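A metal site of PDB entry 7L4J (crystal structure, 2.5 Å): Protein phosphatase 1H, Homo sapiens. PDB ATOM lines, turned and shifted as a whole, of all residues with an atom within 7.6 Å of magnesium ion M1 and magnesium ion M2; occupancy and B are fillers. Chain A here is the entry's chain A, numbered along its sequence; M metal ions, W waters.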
ATOM      1  N   LYS A  60       5.098  17.874 -10.558  1.00  0.00           N
ATOM      2  CA  LYS A  60       5.486  18.712 -11.696  1.00  0.00           C
ATOM      3  C   LYS A  60       4.853  18.281 -13.037  1.00  0.00           C
ATOM      4  O   LYS A  60       5.122  18.935 -14.042  1.00  0.00           O
ATOM      5  CB  LYS A  60       7.010  18.713 -11.827  1.00  0.00           C
ATOM      6  CG  LYS A  60       7.583  17.336 -12.122  1.00  0.00           C
ATOM      7  CD  LYS A  60       9.055  17.384 -12.551  1.00  0.00           C
ATOM      8  CE  LYS A  60       9.409  16.141 -13.386  1.00  0.00           C
ATOM      9  NZ  LYS A  60      10.732  16.197 -14.061  1.00  0.00           N
ATOM     10  N   SER A  61       4.056  17.213 -13.085  1.00  0.00           N
ATOM     11  CA  SER A  61       3.250  16.941 -14.265  1.00  0.00           C
ATOM     12  C   SER A  61       2.163  15.974 -13.855  1.00  0.00           C
ATOM     13  O   SER A  61       2.386  15.107 -13.013  1.00  0.00           O
ATOM     14  CB  SER A  61       4.080  16.386 -15.438  1.00  0.00           C
ATOM     15  OG  SER A  61       4.671  15.129 -15.150  1.00  0.00           O
ATOM     16  N   HIS A  63       0.658  13.506 -15.257  1.00  0.00           N
ATOM     17  CA  HIS A  63       0.913  12.100 -15.522  1.00  0.00           C
ATOM     18  C   HIS A  63       2.363  11.734 -15.232  1.00  0.00           C
ATOM     19  O   HIS A  63       3.271  12.566 -15.324  1.00  0.00           O
ATOM     20  CB  HIS A  63       0.574  11.751 -16.969  1.00  0.00           C
ATOM     21  CG  HIS A  63      -0.894  11.675 -17.242  1.00  0.00           C
ATOM     22  ND1 HIS A  63      -1.427  11.741 -18.510  1.00  0.00           N
ATOM     23  CD2 HIS A  63      -1.939  11.547 -16.397  1.00  0.00           C
ATOM     24  CE1 HIS A  63      -2.737  11.647 -18.435  1.00  0.00           C
ATOM     25  NE2 HIS A  63      -3.074  11.534 -17.161  1.00  0.00           N
ATOM     26  N   ASN A  64       2.571  10.471 -14.842  1.00  0.00           N
ATOM     27  CA  ASN A  64       3.885   9.869 -15.023  1.00  0.00           C
ATOM     28  C   ASN A  64       4.201   9.856 -16.504  1.00  0.00           C
ATOM     29  O   ASN A  64       3.484   9.218 -17.299  1.00  0.00           O
ATOM     30  CB  ASN A  64       3.919   8.441 -14.450  1.00  0.00           C
ATOM     31  CG  ASN A  64       5.351   7.905 -14.298  1.00  0.00           C
ATOM     32  OD1 ASN A  64       6.212   8.142 -15.156  1.00  0.00           O
ATOM     33  ND2 ASN A  64       5.614   7.186 -13.210  1.00  0.00           N
ATOM     34  N   GLU A  65       5.236  10.591 -16.903  1.00  0.00           N
ATOM     35  CA  GLU A  65       5.636  10.708 -18.293  1.00  0.00           C
ATOM     36  C   GLU A  65       6.762   9.765 -18.673  1.00  0.00           C
ATOM     37  O   GLU A  65       7.236   9.821 -19.811  1.00  0.00           O
ATOM     38  CB  GLU A  65       6.020  12.154 -18.628  1.00  0.00           C
ATOM     39  CG  GLU A  65       4.877  13.160 -18.386  1.00  0.00           C
ATOM     40  CD  GLU A  65       5.190  14.551 -18.905  1.00  0.00           C
ATOM     41  OE1 GLU A  65       6.378  14.969 -18.884  1.00  0.00           O
ATOM     42  OE2 GLU A  65       4.239  15.221 -19.352  1.00  0.00           O
ATOM     43  N   ASP A  66       7.226   8.906 -17.761  1.00  0.00           N
ATOM     44  CA  ASP A  66       8.062   7.794 -18.188  1.00  0.00           C
ATOM     45  C   ASP A  66       7.183   6.727 -18.832  1.00  0.00           C
ATOM     46  O   ASP A  66       6.017   6.575 -18.486  1.00  0.00           O
ATOM     47  CB  ASP A  66       8.827   7.153 -17.014  1.00  0.00           C
ATOM     48  CG  ASP A  66      10.005   8.012 -16.495  1.00  0.00           C
ATOM     49  OD1 ASP A  66      10.368   9.078 -17.067  1.00  0.00           O
ATOM     50  OD2 ASP A  66      10.588   7.567 -15.475  1.00  0.00           O
ATOM     51  N   PHE A 122      11.719   5.305 -21.714  1.00  0.00           N
ATOM     52  CA  PHE A 122      11.483   6.583 -22.361  1.00  0.00           C
ATOM     53  C   PHE A 122      11.146   7.573 -21.260  1.00  0.00           C
ATOM     54  O   PHE A 122      10.119   7.400 -20.567  1.00  0.00           O
ATOM     55  CB  PHE A 122      10.351   6.491 -23.371  1.00  0.00           C
ATOM     56  CG  PHE A 122      10.555   5.426 -24.387  1.00  0.00           C
ATOM     57  CD1 PHE A 122      11.368   5.669 -25.484  1.00  0.00           C
ATOM     58  CD2 PHE A 122       9.979   4.170 -24.228  1.00  0.00           C
ATOM     59  CE1 PHE A 122      11.602   4.679 -26.425  1.00  0.00           C
ATOM     60  CE2 PHE A 122      10.225   3.166 -25.152  1.00  0.00           C
ATOM     61  CZ  PHE A 122      11.035   3.434 -26.262  1.00  0.00           C
ATOM     62  N   ASP A 123      11.999   8.573 -21.077  1.00  0.00           N
ATOM     63  CA  ASP A 123      11.680   9.690 -20.200  1.00  0.00           C
ATOM     64  C   ASP A 123      10.980  10.751 -21.042  1.00  0.00           C
ATOM     65  O   ASP A 123      11.613  11.448 -21.842  1.00  0.00           O
ATOM     66  CB  ASP A 123      12.947  10.211 -19.517  1.00  0.00           C
ATOM     67  CG  ASP A 123      12.657  11.223 -18.432  1.00  0.00           C
ATOM     68  OD1 ASP A 123      11.567  11.835 -18.495  1.00  0.00           O
ATOM     69  OD2 ASP A 123      13.498  11.409 -17.532  1.00  0.00           O
ATOM     70  N   GLY A 124       9.666  10.852 -20.915  1.00  0.00           N
ATOM     71  CA  GLY A 124       8.931  11.856 -21.659  1.00  0.00           C
ATOM     72  C   GLY A 124       9.047  13.241 -21.052  1.00  0.00           C
ATOM     73  O   GLY A 124       9.291  13.404 -19.851  1.00  0.00           O
ATOM     74  N   HIS A 125       8.865  14.259 -21.889  1.00  0.00           N
ATOM     75  CA  HIS A 125       8.804  15.628 -21.398  1.00  0.00           C
ATOM     76  C   HIS A 125       7.805  16.408 -22.239  1.00  0.00           C
ATOM     77  O   HIS A 125       7.511  16.064 -23.391  1.00  0.00           O
ATOM     78  CB  HIS A 125      10.181  16.316 -21.422  1.00  0.00           C
ATOM     79  CG  HIS A 125      10.885  16.241 -22.754  1.00  0.00           C
ATOM     80  ND1 HIS A 125      11.920  15.375 -23.012  1.00  0.00           N
ATOM     81  CD2 HIS A 125      10.686  16.948 -23.910  1.00  0.00           C
ATOM     82  CE1 HIS A 125      12.333  15.530 -24.254  1.00  0.00           C
ATOM     83  NE2 HIS A 125      11.604  16.467 -24.820  1.00  0.00           N
ATOM     84  N   ALA A 126       7.255  17.458 -21.608  1.00  0.00           N
ATOM     85  CA  ALA A 126       6.317  18.381 -22.246  1.00  0.00           C
ATOM     86  C   ALA A 126       5.094  17.644 -22.767  1.00  0.00           C
ATOM     87  O   ALA A 126       4.530  18.021 -23.799  1.00  0.00           O
ATOM     88  CB  ALA A 126       6.994  19.165 -23.367  1.00  0.00           C
ATOM     89  N   GLY A 127       4.688  16.581 -22.057  1.00  0.00           N
ATOM     90  CA  GLY A 127       3.620  15.727 -22.514  1.00  0.00           C
ATOM     91  C   GLY A 127       4.009  14.254 -22.489  1.00  0.00           C
ATOM     92  O   GLY A 127       5.188  13.911 -22.406  1.00  0.00           O
ATOM     93  N   GLY A 205       8.144  15.334 -26.201  1.00  0.00           N
ATOM     94  CA  GLY A 205       9.299  14.589 -26.623  1.00  0.00           C
ATOM     95  C   GLY A 205       9.602  13.537 -25.569  1.00  0.00           C
ATOM     96  O   GLY A 205       8.956  13.498 -24.517  1.00  0.00           O
ATOM     97  N   CYS A 206      10.574  12.695 -25.861  1.00  0.00           N
ATOM     98  CA  CYS A 206      11.061  11.789 -24.828  1.00  0.00           C
ATOM     99  C   CYS A 206      12.488  11.361 -25.145  1.00  0.00           C
ATOM    100  O   CYS A 206      12.942  11.408 -26.296  1.00  0.00           O
ATOM    101  CB  CYS A 206      10.128  10.575 -24.710  1.00  0.00           C
ATOM    102  SG  CYS A 206      10.200   9.504 -26.250  1.00  0.00           S
ATOM    103  N   THR A 207      13.201  10.999 -24.102  1.00  0.00           N
ATOM    104  CA  THR A 207      14.465  10.315 -24.276  1.00  0.00           C
ATOM    105  C   THR A 207      14.185   8.840 -24.572  1.00  0.00           C
ATOM    106  O   THR A 207      13.072   8.354 -24.417  1.00  0.00           O
ATOM    107  CB  THR A 207      15.326  10.460 -23.012  1.00  0.00           C
ATOM    108  OG1 THR A 207      14.661   9.827 -21.927  1.00  0.00           O
ATOM    109  CG2 THR A 207      15.495  11.931 -22.683  1.00  0.00           C
ATOM    110  N   ASP A 225      19.222  11.194 -21.369  1.00  0.00           N
ATOM    111  CA  ASP A 225      19.968  11.201 -20.114  1.00  0.00           C
ATOM    112  C   ASP A 225      19.478  10.136 -19.130  1.00  0.00           C
ATOM    113  O   ASP A 225      19.652  10.299 -17.927  1.00  0.00           O
ATOM    114  CB  ASP A 225      19.923  12.581 -19.453  1.00  0.00           C
ATOM    115  CG  ASP A 225      18.507  13.097 -19.244  1.00  0.00           C
ATOM    116  OD1 ASP A 225      17.533  12.358 -19.530  1.00  0.00           O
ATOM    117  OD2 ASP A 225      18.370  14.259 -18.797  1.00  0.00           O
ATOM    118  N   SER A 226      18.816   9.087 -19.616  1.00  0.00           N
ATOM    119  CA  SER A 226      18.718   7.882 -18.801  1.00  0.00           C
ATOM    120  C   SER A 226      20.088   7.216 -18.763  1.00  0.00           C
ATOM    121  O   SER A 226      21.017   7.616 -19.476  1.00  0.00           O
ATOM    122  CB  SER A 226      17.652   6.943 -19.390  1.00  0.00           C
ATOM    123  OG  SER A 226      16.325   7.382 -19.072  1.00  0.00           O
ATOM    124  N   LYS A 315      22.128  20.001 -14.001  1.00  0.00           N
ATOM    125  CA  LYS A 315      20.837  19.844 -14.640  1.00  0.00           C
ATOM    126  C   LYS A 315      20.126  21.166 -14.884  1.00  0.00           C
ATOM    127  O   LYS A 315      19.077  21.177 -15.528  1.00  0.00           O
ATOM    128  CB  LYS A 315      19.939  18.915 -13.813  1.00  0.00           C
ATOM    129  CG  LYS A 315      20.368  17.465 -13.876  1.00  0.00           C
ATOM    130  CD  LYS A 315      19.226  16.535 -13.536  1.00  0.00           C
ATOM    131  CE  LYS A 315      18.339  16.189 -14.748  1.00  0.00           C
ATOM    132  NZ  LYS A 315      18.668  14.877 -15.406  1.00  0.00           N
ATOM    133  N   THR A 373      15.650   5.793 -15.646  1.00  0.00           N
ATOM    134  CA  THR A 373      15.530   7.169 -16.055  1.00  0.00           C
ATOM    135  C   THR A 373      16.274   8.065 -15.063  1.00  0.00           C
ATOM    136  O   THR A 373      16.621   7.637 -13.959  1.00  0.00           O
ATOM    137  CB  THR A 373      14.062   7.573 -16.143  1.00  0.00           C
ATOM    138  OG1 THR A 373      13.417   7.263 -14.904  1.00  0.00           O
ATOM    139  CG2 THR A 373      13.366   6.809 -17.294  1.00  0.00           C
ATOM    140  N   ASP A 374      16.499   9.329 -15.453  1.00  0.00           N
ATOM    141  CA  ASP A 374      17.263  10.232 -14.574  1.00  0.00           C
ATOM    142  C   ASP A 374      16.583  10.445 -13.231  1.00  0.00           C
ATOM    143  O   ASP A 374      17.253  10.872 -12.291  1.00  0.00           O
ATOM    144  CB  ASP A 374      17.532  11.588 -15.230  1.00  0.00           C
ATOM    145  CG  ASP A 374      16.268  12.344 -15.641  1.00  0.00           C
ATOM    146  OD1 ASP A 374      15.147  11.911 -15.291  1.00  0.00           O
ATOM    147  OD2 ASP A 374      16.404  13.387 -16.330  1.00  0.00           O
ATOM    148  N   GLY A 375      15.289  10.140 -13.118  1.00  0.00           N
ATOM    149  CA  GLY A 375      14.651  10.169 -11.813  1.00  0.00           C
ATOM    150  C   GLY A 375      15.460   9.433 -10.755  1.00  0.00           C
ATOM    151  O   GLY A 375      15.437   9.812  -9.573  1.00  0.00           O
ATOM    152  N   LEU A 376      16.186   8.391 -11.146  1.00  0.00           N
ATOM    153  CA  LEU A 376      17.064   7.684 -10.217  1.00  0.00           C
ATOM    154  C   LEU A 376      18.448   8.311 -10.144  1.00  0.00           C
ATOM    155  O   LEU A 376      18.917   8.630  -9.046  1.00  0.00           O
ATOM    156  CB  LEU A 376      17.188   6.209 -10.616  1.00  0.00           C
ATOM    157  CG  LEU A 376      17.762   5.247  -9.572  1.00  0.00           C
ATOM    158  CD1 LEU A 376      16.652   4.659  -8.704  1.00  0.00           C
ATOM    159  CD2 LEU A 376      18.550   4.149 -10.255  1.00  0.00           C
ATOM    160  N   ASP A 378      19.630  11.189 -10.735  1.00  0.00           N
ATOM    161  CA  ASP A 378      19.770  12.556 -10.261  1.00  0.00           C
ATOM    162  C   ASP A 378      20.010  12.630  -8.752  1.00  0.00           C
ATOM    163  O   ASP A 378      20.494  13.656  -8.269  1.00  0.00           O
ATOM    164  CB  ASP A 378      18.538  13.374 -10.622  1.00  0.00           C
ATOM    165  CG  ASP A 378      18.444  13.662 -12.113  1.00  0.00           C
ATOM    166  OD1 ASP A 378      19.492  13.582 -12.804  1.00  0.00           O
ATOM    167  OD2 ASP A 378      17.327  13.961 -12.590  1.00  0.00           O
ATOM    168  N   SER A 433      14.294  12.453  -4.946  1.00  0.00           N
ATOM    169  CA  SER A 433      13.904  12.681  -6.333  1.00  0.00           C
ATOM    170  C   SER A 433      12.422  13.039  -6.447  1.00  0.00           C
ATOM    171  O   SER A 433      11.554  12.323  -5.940  1.00  0.00           O
ATOM    172  CB  SER A 433      14.207  11.446  -7.175  1.00  0.00           C
ATOM    173  OG  SER A 433      14.032  11.729  -8.551  1.00  0.00           O
ATOM    174  N   ASP A 435      11.134  13.573  -9.563  1.00  0.00           N
ATOM    175  CA  ASP A 435      10.837  13.192 -10.927  1.00  0.00           C
ATOM    176  C   ASP A 435      10.103  11.851 -10.959  1.00  0.00           C
ATOM    177  O   ASP A 435      10.003  11.144  -9.954  1.00  0.00           O
ATOM    178  CB  ASP A 435      12.137  13.125 -11.725  1.00  0.00           C
ATOM    179  CG  ASP A 435      11.904  13.068 -13.217  1.00  0.00           C
ATOM    180  OD1 ASP A 435      10.736  13.199 -13.652  1.00  0.00           O
ATOM    181  OD2 ASP A 435      12.897  12.860 -13.958  1.00  0.00           O
ATOM    182  N   ASP A 436       9.578  11.508 -12.137  1.00  0.00           N
ATOM    183  CA  ASP A 436       9.195  10.130 -12.410  1.00  0.00           C
ATOM    184  C   ASP A 436      10.438   9.252 -12.320  1.00  0.00           C
ATOM    185  O   ASP A 436      11.518   9.631 -12.813  1.00  0.00           O
ATOM    186  CB  ASP A 436       8.557   9.987 -13.794  1.00  0.00           C
ATOM    187  CG  ASP A 436       7.342  10.902 -13.988  1.00  0.00           C
ATOM    188  OD1 ASP A 436       6.474  10.965 -13.076  1.00  0.00           O
ATOM    189  OD2 ASP A 436       7.238  11.554 -15.069  1.00  0.00           O
ATOM    190  N   ILE A 437      10.314   8.115 -11.661  1.00  0.00           N
ATOM    191  CA  ILE A 437      11.396   7.148 -11.554  1.00  0.00           C
ATOM    192  C   ILE A 437      10.910   5.827 -12.142  1.00  0.00           C
ATOM    193  O   ILE A 437       9.846   5.333 -11.749  1.00  0.00           O
ATOM    194  CB  ILE A 437      11.870   6.972 -10.099  1.00  0.00           C
ATOM    195  CG1 ILE A 437      12.076   8.350  -9.434  1.00  0.00           C
ATOM    196  CG2 ILE A 437      13.124   6.086 -10.044  1.00  0.00           C
ATOM    197  CD1 ILE A 437      12.224   8.272  -7.919  1.00  0.00           C
HETATM  198 MG    MG M   1      13.153  12.297 -15.792  1.00  0.00          MG
HETATM  199 MG    MG M   2      10.269  13.173 -17.964  1.00  0.00          MG
HETATM  200  O   HOH W   1      13.774  14.115 -16.760  1.00  0.00           O
HETATM  201  O   HOH W   2      11.773  14.511 -18.938  1.00  0.00           O
HETATM  202  O   HOH W   3       8.710  14.473 -17.219  1.00  0.00           O
HETATM  203  O   HOH W   4       9.159  11.330 -17.108  1.00  0.00           O
HETATM  204  O   HOH W   5      11.163  13.142 -16.168  1.00  0.00           O
HETATM  205  O   HOH W   6      12.253  10.499 -15.157  1.00  0.00           O
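Of the 27 residues printed, 3 come within 4 Å of magnesium ion M1.
Magnesium ion M1 is bound by the side-chain carboxylate (OD2) of Asp 435 (1.9 Å), the side-chain carboxylate (OD2) of Asp 123 (2.0 Å), the side-chain carboxylate (OD1) of Asp 374 (2.1 Å), water W6 (2.1 Å), water W1 (2.2 Å) and water W5 (2.2 Å). Magnesium ion M1 has six donor atoms within binding distance.
Water W4 bridges the side-chain carboxylate (OD1) of Asp 66 (2.6 Å) and the side-chain carboxylate (OD2) of Asp 436 (2.8 Å).
The side-chain amino group (NZ) of Lys 315 is in salt-bridge range of the side-chain carboxylate (OD2) of Asp 374 (2.9 Å). The backbone NH of Gly 124 lies within hydrogen-bond range of the backbone carbonyl oxygen of Glu 65, at 2.9 Å. N of Thr 207 is in hydrogen-bond range of O of Asp 123. The side-chain carboxylate (OD1) of Asp 435 is in salt-bridge range of the side-chain amino group (NZ) of Lys 60 (3.0 Å).
Magnesium ion M2 is bound by OD1 of Asp 123 (1.9 Å). Magnesium ion M2 is bound by water W5, at 2.0 Å. Magnesium ion M2 is bound by O of Gly 124 (2.1 Å). Water W3 binds magnesium ion M2 (2.2 Å). Water W2 is bound to magnesium ion M2 (2.2 Å). Water W4 is bound to magnesium ion M2 (2.3 Å). Magnesium ion M2 has six donor atoms within binding distance.
Of the 27 residues printed, 2 come within 4 Å of magnesium ion M2.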
